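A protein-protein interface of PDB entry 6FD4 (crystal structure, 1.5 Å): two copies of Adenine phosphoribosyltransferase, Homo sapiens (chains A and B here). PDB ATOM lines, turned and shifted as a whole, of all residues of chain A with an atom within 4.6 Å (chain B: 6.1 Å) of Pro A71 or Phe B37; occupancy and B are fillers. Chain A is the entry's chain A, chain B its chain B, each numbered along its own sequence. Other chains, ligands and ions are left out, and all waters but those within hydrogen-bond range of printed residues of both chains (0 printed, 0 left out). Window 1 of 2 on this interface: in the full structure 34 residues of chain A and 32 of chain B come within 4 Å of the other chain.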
ATOM      1  N   PHE A  67     -24.254  12.768 -23.804  1.00  0.00           N
ATOM      2  CA  PHE A  67     -23.525  12.588 -25.062  1.00  0.00           C
ATOM      3  C   PHE A  67     -22.363  13.564 -25.192  1.00  0.00           C
ATOM      4  O   PHE A  67     -21.434  13.315 -25.948  1.00  0.00           O
ATOM      5  CB  PHE A  67     -24.461  12.800 -26.253  1.00  0.00           C
ATOM      6  CG  PHE A  67     -25.406  11.663 -26.551  1.00  0.00           C
ATOM      7  CD1 PHE A  67     -25.439  10.510 -25.786  1.00  0.00           C
ATOM      8  CD2 PHE A  67     -26.296  11.786 -27.587  1.00  0.00           C
ATOM      9  CE1 PHE A  67     -26.290   9.475 -26.120  1.00  0.00           C
ATOM     10  CE2 PHE A  67     -27.178  10.764 -27.907  1.00  0.00           C
ATOM     11  CZ  PHE A  67     -27.144   9.601 -27.182  1.00  0.00           C
ATOM     12  N   PHE A  69     -20.291  14.275 -22.935  1.00  0.00           N
ATOM     13  CA  PHE A  69     -19.159  13.818 -22.126  1.00  0.00           C
ATOM     14  C   PHE A  69     -18.740  12.392 -22.407  1.00  0.00           C
ATOM     15  O   PHE A  69     -17.549  12.054 -22.269  1.00  0.00           O
ATOM     16  CB  PHE A  69     -19.494  13.987 -20.641  1.00  0.00           C
ATOM     17  CG  PHE A  69     -19.775  15.417 -20.265  1.00  0.00           C
ATOM     18  CD1 PHE A  69     -18.729  16.304 -20.060  1.00  0.00           C
ATOM     19  CD2 PHE A  69     -21.072  15.895 -20.250  1.00  0.00           C
ATOM     20  CE1 PHE A  69     -18.969  17.638 -19.783  1.00  0.00           C
ATOM     21  CE2 PHE A  69     -21.322  17.222 -19.966  1.00  0.00           C
ATOM     22  CZ  PHE A  69     -20.279  18.099 -19.738  1.00  0.00           C
ATOM     23  N   GLY A  70     -19.683  11.547 -22.818  1.00  0.00           N
ATOM     24  CA  GLY A  70     -19.361  10.103 -22.973  1.00  0.00           C
ATOM     25  C   GLY A  70     -18.200   9.796 -23.909  1.00  0.00           C
ATOM     26  O   GLY A  70     -17.242   9.091 -23.531  1.00  0.00           O
ATOM     27  N   PRO A  71     -18.250  10.304 -25.142  1.00  0.00           N
ATOM     28  CA  PRO A  71     -17.195   9.970 -26.077  1.00  0.00           C
ATOM     29  C   PRO A  71     -15.832  10.503 -25.667  1.00  0.00           C
ATOM     30  O   PRO A  71     -14.835   9.782 -25.763  1.00  0.00           O
ATOM     31  CB  PRO A  71     -17.688  10.565 -27.396  1.00  0.00           C
ATOM     32  CG  PRO A  71     -19.171  10.587 -27.255  1.00  0.00           C
ATOM     33  CD  PRO A  71     -19.415  10.911 -25.815  1.00  0.00           C
ATOM     34  N   SER A  72     -15.757  11.724 -25.152  1.00  0.00           N
ATOM     35  CA  SER A  72     -14.467  12.257 -24.724  1.00  0.00           C
ATOM     36  C   SER A  72     -13.908  11.486 -23.541  1.00  0.00           C
ATOM     37  O   SER A  72     -12.715  11.247 -23.450  1.00  0.00           O
ATOM     38  CB  SER A  72     -14.565  13.738 -24.364  1.00  0.00           C
ATOM     39  OG  SER A  72     -14.823  14.530 -25.528  1.00  0.00           O
ATOM     40  N   LEU A  73     -14.776  11.107 -22.622  1.00  0.00           N
ATOM     41  CA  LEU A  73     -14.340  10.321 -21.471  1.00  0.00           C
ATOM     42  C   LEU A  73     -13.839   8.957 -21.898  1.00  0.00           C
ATOM     43  O   LEU A  73     -12.763   8.515 -21.476  1.00  0.00           O
ATOM     44  CB  LEU A  73     -15.448  10.207 -20.440  1.00  0.00           C
ATOM     45  CG  LEU A  73     -15.135   9.433 -19.151  1.00  0.00           C
ATOM     46  CD1 LEU A  73     -13.902  10.003 -18.439  1.00  0.00           C
ATOM     47  CD2 LEU A  73     -16.362   9.407 -18.246  1.00  0.00           C
ATOM     48  N   ALA A  74     -14.597   8.299 -22.759  1.00  0.00           N
ATOM     49  CA  ALA A  74     -14.192   7.023 -23.304  1.00  0.00           C
ATOM     50  C   ALA A  74     -12.838   7.131 -23.994  1.00  0.00           C
ATOM     51  O   ALA A  74     -11.920   6.346 -23.701  1.00  0.00           O
ATOM     52  CB  ALA A  74     -15.256   6.486 -24.274  1.00  0.00           C
ATOM     53  N   GLN A  75     -12.680   8.127 -24.855  1.00  0.00           N
ATOM     54  CA  GLN A  75     -11.436   8.328 -25.553  1.00  0.00           C
ATOM     55  C   GLN A  75     -10.257   8.512 -24.607  1.00  0.00           C
ATOM     56  O   GLN A  75      -9.193   7.935 -24.815  1.00  0.00           O
ATOM     57  CB  GLN A  75     -11.555   9.522 -26.471  1.00  0.00           C
ATOM     58  CG  GLN A  75     -12.275   9.194 -27.762  1.00  0.00           C
ATOM     59  CD  GLN A  75     -11.389   8.466 -28.748  1.00  0.00           C
ATOM     60  OE1 GLN A  75     -10.354   8.979 -29.174  1.00  0.00           O
ATOM     61  NE2 GLN A  75     -11.785   7.260 -29.117  1.00  0.00           N
ATOM     62  N   CYS A  81     -17.602   3.945 -26.454  1.00  0.00           N
ATOM     63  CA  CYS A  81     -18.776   4.507 -25.815  1.00  0.00           C
ATOM     64  C   CYS A  81     -20.024   3.908 -26.453  1.00  0.00           C
ATOM     65  O   CYS A  81     -20.181   3.908 -27.677  1.00  0.00           O
ATOM     66  CB  CYS A  81     -18.768   6.029 -25.987  1.00  0.00           C
ATOM     67  SG  CYS A  81     -20.073   6.903 -25.091  1.00  0.00           S
ATOM     68  N   VAL B   7     -13.765   4.179 -40.296  1.00  0.00           N
ATOM     69  CA  VAL B   7     -15.083   4.756 -40.084  1.00  0.00           C
ATOM     70  C   VAL B   7     -16.154   4.052 -40.921  1.00  0.00           C
ATOM     71  O   VAL B   7     -17.193   3.638 -40.400  1.00  0.00           O
ATOM     72  CB  VAL B   7     -15.078   6.269 -40.380  1.00  0.00           C
ATOM     73  CG1 VAL B   7     -16.402   6.917 -39.985  1.00  0.00           C
ATOM     74  CG2 VAL B   7     -13.896   6.939 -39.686  1.00  0.00           C
ATOM     75  N   VAL B  30     -19.261   3.216 -34.678  1.00  0.00           N
ATOM     76  CA  VAL B  30     -18.152   4.159 -34.729  1.00  0.00           C
ATOM     77  C   VAL B  30     -17.830   4.626 -33.310  1.00  0.00           C
ATOM     78  O   VAL B  30     -16.670   4.651 -32.906  1.00  0.00           O
ATOM     79  CB  VAL B  30     -18.465   5.392 -35.595  1.00  0.00           C
ATOM     80  CG1 VAL B  30     -17.329   6.382 -35.490  1.00  0.00           C
ATOM     81  CG2 VAL B  30     -18.738   5.002 -37.041  1.00  0.00           C
ATOM     82  N   LEU B  31     -18.868   4.910 -32.530  1.00  0.00           N
ATOM     83  CA  LEU B  31     -18.660   5.387 -31.151  1.00  0.00           C
ATOM     84  C   LEU B  31     -18.104   4.271 -30.249  1.00  0.00           C
ATOM     85  O   LEU B  31     -17.320   4.532 -29.332  1.00  0.00           O
ATOM     86  CB  LEU B  31     -19.970   5.910 -30.557  1.00  0.00           C
ATOM     87  CG  LEU B  31     -20.393   7.359 -30.873  1.00  0.00           C
ATOM     88  CD1 LEU B  31     -19.589   8.372 -30.063  1.00  0.00           C
ATOM     89  CD2 LEU B  31     -20.260   7.676 -32.341  1.00  0.00           C
ATOM     90  N   LYS B  32     -18.510   3.042 -30.534  1.00  0.00           N
ATOM     91  CA  LYS B  32     -18.110   1.884 -29.736  1.00  0.00           C
ATOM     92  C   LYS B  32     -16.674   1.402 -29.939  1.00  0.00           C
ATOM     93  O   LYS B  32     -16.092   0.765 -29.063  1.00  0.00           O
ATOM     94  CB  LYS B  32     -19.073   0.724 -30.008  1.00  0.00           C
ATOM     95  CG  LYS B  32     -18.923  -0.421 -29.032  1.00  0.00           C
ATOM     96  CD  LYS B  32     -20.039  -1.437 -29.190  1.00  0.00           C
ATOM     97  CE  LYS B  32     -19.820  -2.617 -28.271  1.00  0.00           C
ATOM     98  NZ  LYS B  32     -20.895  -3.626 -28.444  1.00  0.00           N
ATOM     99  N   ASP B  33     -16.102   1.701 -31.111  1.00  0.00           N
ATOM    100  CA  ASP B  33     -14.745   1.300 -31.439  1.00  0.00           C
ATOM    101  C   ASP B  33     -13.874   2.546 -31.306  1.00  0.00           C
ATOM    102  O   ASP B  33     -13.996   3.483 -32.101  1.00  0.00           O
ATOM    103  CB  ASP B  33     -14.732   0.724 -32.862  1.00  0.00           C
ATOM    104  CG  ASP B  33     -13.350   0.426 -33.379  1.00  0.00           C
ATOM    105  OD1 ASP B  33     -12.353   0.745 -32.695  1.00  0.00           O
ATOM    106  OD2 ASP B  33     -13.266  -0.112 -34.515  1.00  0.00           O
ATOM    107  N   PRO B  34     -13.052   2.614 -30.251  1.00  0.00           N
ATOM    108  CA  PRO B  34     -12.338   3.862 -30.044  1.00  0.00           C
ATOM    109  C   PRO B  34     -11.446   4.259 -31.209  1.00  0.00           C
ATOM    110  O   PRO B  34     -11.210   5.453 -31.421  1.00  0.00           O
ATOM    111  CB  PRO B  34     -11.526   3.614 -28.774  1.00  0.00           C
ATOM    112  CG  PRO B  34     -11.434   2.119 -28.654  1.00  0.00           C
ATOM    113  CD  PRO B  34     -12.684   1.578 -29.269  1.00  0.00           C
ATOM    114  N   ALA B  35     -10.935   3.284 -31.957  1.00  0.00           N
ATOM    115  CA  ALA B  35     -10.066   3.613 -33.089  1.00  0.00           C
ATOM    116  C   ALA B  35     -10.865   4.282 -34.214  1.00  0.00           C
ATOM    117  O   ALA B  35     -10.358   5.189 -34.917  1.00  0.00           O
ATOM    118  CB  ALA B  35      -9.382   2.360 -33.608  1.00  0.00           C
ATOM    119  N   SER B  36     -12.101   3.841 -34.379  1.00  0.00           N
ATOM    120  CA  SER B  36     -12.989   4.370 -35.401  1.00  0.00           C
ATOM    121  C   SER B  36     -13.400   5.795 -35.058  1.00  0.00           C
ATOM    122  O   SER B  36     -13.386   6.690 -35.904  1.00  0.00           O
ATOM    123  CB  SER B  36     -14.223   3.470 -35.513  1.00  0.00           C
ATOM    124  OG  SER B  36     -15.049   3.845 -36.586  1.00  0.00           O
ATOM    125  N   PHE B  37     -13.750   6.009 -33.797  1.00  0.00           N
ATOM    126  CA  PHE B  37     -14.144   7.345 -33.359  1.00  0.00           C
ATOM    127  C   PHE B  37     -12.972   8.313 -33.506  1.00  0.00           C
ATOM    128  O   PHE B  37     -13.130   9.446 -34.014  1.00  0.00           O
ATOM    129  CB  PHE B  37     -14.628   7.322 -31.911  1.00  0.00           C
ATOM    130  CG  PHE B  37     -15.134   8.652 -31.424  1.00  0.00           C
ATOM    131  CD1 PHE B  37     -16.369   9.115 -31.824  1.00  0.00           C
ATOM    132  CD2 PHE B  37     -14.370   9.443 -30.593  1.00  0.00           C
ATOM    133  CE1 PHE B  37     -16.849  10.327 -31.387  1.00  0.00           C
ATOM    134  CE2 PHE B  37     -14.840  10.685 -30.170  1.00  0.00           C
ATOM    135  CZ  PHE B  37     -16.086  11.106 -30.561  1.00  0.00           C
ATOM    136  N   ARG B  38     -11.786   7.894 -33.076  1.00  0.00           N
ATOM    137  CA  ARG B  38     -10.613   8.746 -33.166  1.00  0.00           C
ATOM    138  C   ARG B  38     -10.330   9.078 -34.621  1.00  0.00           C
ATOM    139  O   ARG B  38      -9.968  10.215 -34.951  1.00  0.00           O
ATOM    140  CB  ARG B  38      -9.411   8.056 -32.516  1.00  0.00           C
ATOM    141  CG  ARG B  38      -8.124   8.871 -32.524  1.00  0.00           C
ATOM    142  CD  ARG B  38      -7.073   8.242 -31.613  1.00  0.00           C
ATOM    143  NE  ARG B  38      -6.973   6.789 -31.784  1.00  0.00           N
ATOM    144  CZ  ARG B  38      -7.203   5.897 -30.817  1.00  0.00           C
ATOM    145  NH1 ARG B  38      -7.089   4.596 -31.067  1.00  0.00           N
ATOM    146  NH2 ARG B  38      -7.546   6.301 -29.599  1.00  0.00           N
ATOM    147  N   ALA B  39     -10.524   8.103 -35.507  1.00  0.00           N
ATOM    148  CA  ALA B  39     -10.294   8.362 -36.917  1.00  0.00           C
ATOM    149  C   ALA B  39     -11.276   9.403 -37.442  1.00  0.00           C
ATOM    150  O   ALA B  39     -10.887  10.301 -38.202  1.00  0.00           O
ATOM    151  CB  ALA B  39     -10.382   7.076 -37.725  1.00  0.00           C
ATOM    152  N   ALA B  40     -12.557   9.255 -37.103  1.00  0.00           N
ATOM    153  CA  ALA B  40     -13.567  10.193 -37.583  1.00  0.00           C
ATOM    154  C   ALA B  40     -13.229  11.619 -37.142  1.00  0.00           C
ATOM    155  O   ALA B  40     -13.263  12.563 -37.942  1.00  0.00           O
ATOM    156  CB  ALA B  40     -14.918   9.773 -37.055  1.00  0.00           C
ATOM    157  N   ILE B  41     -12.911  11.782 -35.866  1.00  0.00           N
ATOM    158  CA  ILE B  41     -12.593  13.111 -35.337  1.00  0.00           C
ATOM    159  C   ILE B  41     -11.345  13.651 -36.041  1.00  0.00           C
ATOM    160  O   ILE B  41     -11.289  14.817 -36.438  1.00  0.00           O
ATOM    161  CB  ILE B  41     -12.403  13.061 -33.811  1.00  0.00           C
ATOM    162  CG1 ILE B  41     -13.724  12.690 -33.114  1.00  0.00           C
ATOM    163  CG2 ILE B  41     -11.890  14.391 -33.254  1.00  0.00           C
ATOM    164  CD1 ILE B  41     -14.876  13.614 -33.434  1.00  0.00           C
ATOM    165  N   GLY B  42     -10.353  12.792 -36.226  1.00  0.00           N
ATOM    166  CA  GLY B  42      -9.105  13.206 -36.840  1.00  0.00           C
ATOM    167  C   GLY B  42      -9.280  13.627 -38.287  1.00  0.00           C
ATOM    168  O   GLY B  42      -8.668  14.607 -38.721  1.00  0.00           O
ATOM    169  N   PHE B  67     -23.933  16.168 -30.551  1.00  0.00           N
ATOM    170  CA  PHE B  67     -23.259  16.320 -29.265  1.00  0.00           C
ATOM    171  C   PHE B  67     -22.180  15.249 -29.098  1.00  0.00           C
ATOM    172  O   PHE B  67     -21.259  15.414 -28.331  1.00  0.00           O
ATOM    173  CB  PHE B  67     -24.258  16.182 -28.091  1.00  0.00           C
ATOM    174  CG  PHE B  67     -25.165  17.370 -27.859  1.00  0.00           C
ATOM    175  CD1 PHE B  67     -25.054  18.548 -28.590  1.00  0.00           C
ATOM    176  CD2 PHE B  67     -26.108  17.307 -26.852  1.00  0.00           C
ATOM    177  CE1 PHE B  67     -25.867  19.634 -28.310  1.00  0.00           C
ATOM    178  CE2 PHE B  67     -26.924  18.390 -26.570  1.00  0.00           C
ATOM    179  CZ  PHE B  67     -26.796  19.552 -27.308  1.00  0.00           C
ATOM    180  N   LEU B  68     -22.341  14.126 -29.782  1.00  0.00           N
ATOM    181  CA  LEU B  68     -21.368  13.044 -29.693  1.00  0.00           C
ATOM    182  C   LEU B  68     -20.047  13.417 -30.360  1.00  0.00           C
ATOM    183  O   LEU B  68     -19.002  12.827 -30.045  1.00  0.00           O
ATOM    184  CB  LEU B  68     -21.908  11.772 -30.348  1.00  0.00           C
ATOM    185  CG  LEU B  68     -23.108  11.142 -29.637  1.00  0.00           C
ATOM    186  CD1 LEU B  68     -23.745  10.158 -30.600  1.00  0.00           C
ATOM    187  CD2 LEU B  68     -22.720  10.444 -28.341  1.00  0.00           C
ATOM    188  N   PHE B  69     -20.089  14.351 -31.301  1.00  0.00           N
ATOM    189  CA  PHE B  69     -18.896  14.701 -32.068  1.00  0.00           C
ATOM    190  C   PHE B  69     -18.360  16.112 -31.776  1.00  0.00           C
ATOM    191  O   PHE B  69     -17.146  16.336 -31.815  1.00  0.00           O
ATOM    192  CB  PHE B  69     -19.178  14.520 -33.559  1.00  0.00           C
ATOM    193  CG  PHE B  69     -19.545  13.120 -33.926  1.00  0.00           C
ATOM    194  CD1 PHE B  69     -18.579  12.162 -34.154  1.00  0.00           C
ATOM    195  CD2 PHE B  69     -20.877  12.742 -33.955  1.00  0.00           C
ATOM    196  CE1 PHE B  69     -18.929  10.852 -34.453  1.00  0.00           C
ATOM    197  CE2 PHE B  69     -21.224  11.440 -34.220  1.00  0.00           C
ATOM    198  CZ  PHE B  69     -20.260  10.489 -34.478  1.00  0.00           C
ATOM    199  N   SER B  72     -15.531  16.576 -28.911  1.00  0.00           N
ATOM    200  CA  SER B  72     -14.267  15.918 -29.248  1.00  0.00           C
ATOM    201  C   SER B  72     -13.567  16.644 -30.401  1.00  0.00           C
ATOM    202  O   SER B  72     -12.339  16.788 -30.408  1.00  0.00           O
ATOM    203  CB  SER B  72     -14.486  14.450 -29.634  1.00  0.00           C
ATOM    204  OG  SER B  72     -14.927  13.665 -28.510  1.00  0.00           O
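The backbone NH (N) of Phe B37 lies within hydrogen-bond range of the backbone carbonyl oxygen (O) of Val B30, at 3.3 Å.
Hydrophobic or aromatic side chains of chain B that line the printed part of chain A: Leu B31, Pro B34, Phe B37, Phe B67 and Leu B68.
Of the 9 printed residues of chain A, 5 touch a printed residue of chain B.
Hydrophobic or aromatic side chains of chain A within 4 Å of the printed part of chain B: Phe A67 and Pro A71.
Among the printed residues, 11 pairs touch across the chains.
Of chain B, only Leu B31, Phe B37 and Leu B68 come within 4 Å of Pro A71.
Phe B37 touches two residues of chain A.
Printed residues of chain A within 4 Å of Ser B72: Ser A72 (3.1 Å).
Of the printed residues of chain A, Leu B31 touches Pro A71 (3.6 Å) and Cys A81 (3.0 Å).
Printed residues of chain B within 4 Å of Cys A81: Leu B31 (3.0 Å) and Lys B32 (3.4 Å).
The nearest printed residue of chain A that does not touch Pro B34 is Ala A74 (5.8 Å).
Phe B67 touches its own counterpart, Phe A67.
Ser B72 touches its own counterpart, Ser A72.
Positions printed for both chains: 67, 69 and 72.
Among the printed residues, merely in contact across the chains: Phe A67 with Leu B68 (3.5 Å), Gln A75 with Phe B37 (3.5 Å), Pro A71 with Leu B68 (3.6 Å), Pro A71 with Phe B37 (3.6 Å), Gln A75 with Arg B38 (3.6 Å) and Pro A71 with Leu B31 (3.6 Å).
The backbone carbonyl oxygen (O) of Phe B67 lies close to the backbone carbonyl oxygen (O) of Phe A67 (3.2 Å).
The backbone carbonyl oxygen (O) of Leu B31 is in hydrogen-bond range of the backbone NH (N) of Cys A81 (3.0 Å).
The backbone NH (N) of Lys B32 lies within hydrogen-bond range of the backbone carbonyl oxygen (O) of Cys A81 (3.4 Å).
The side-chain hydroxyl of Ser A72 lies within hydrogen-bond range of the side-chain hydroxyl of Ser B72, 3.1 Å away.
The side-chain amide nitrogen of Gln A75 sits at hydrogen-bond distance from the backbone carbonyl oxygen of Pro B34 (3.0 Å).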
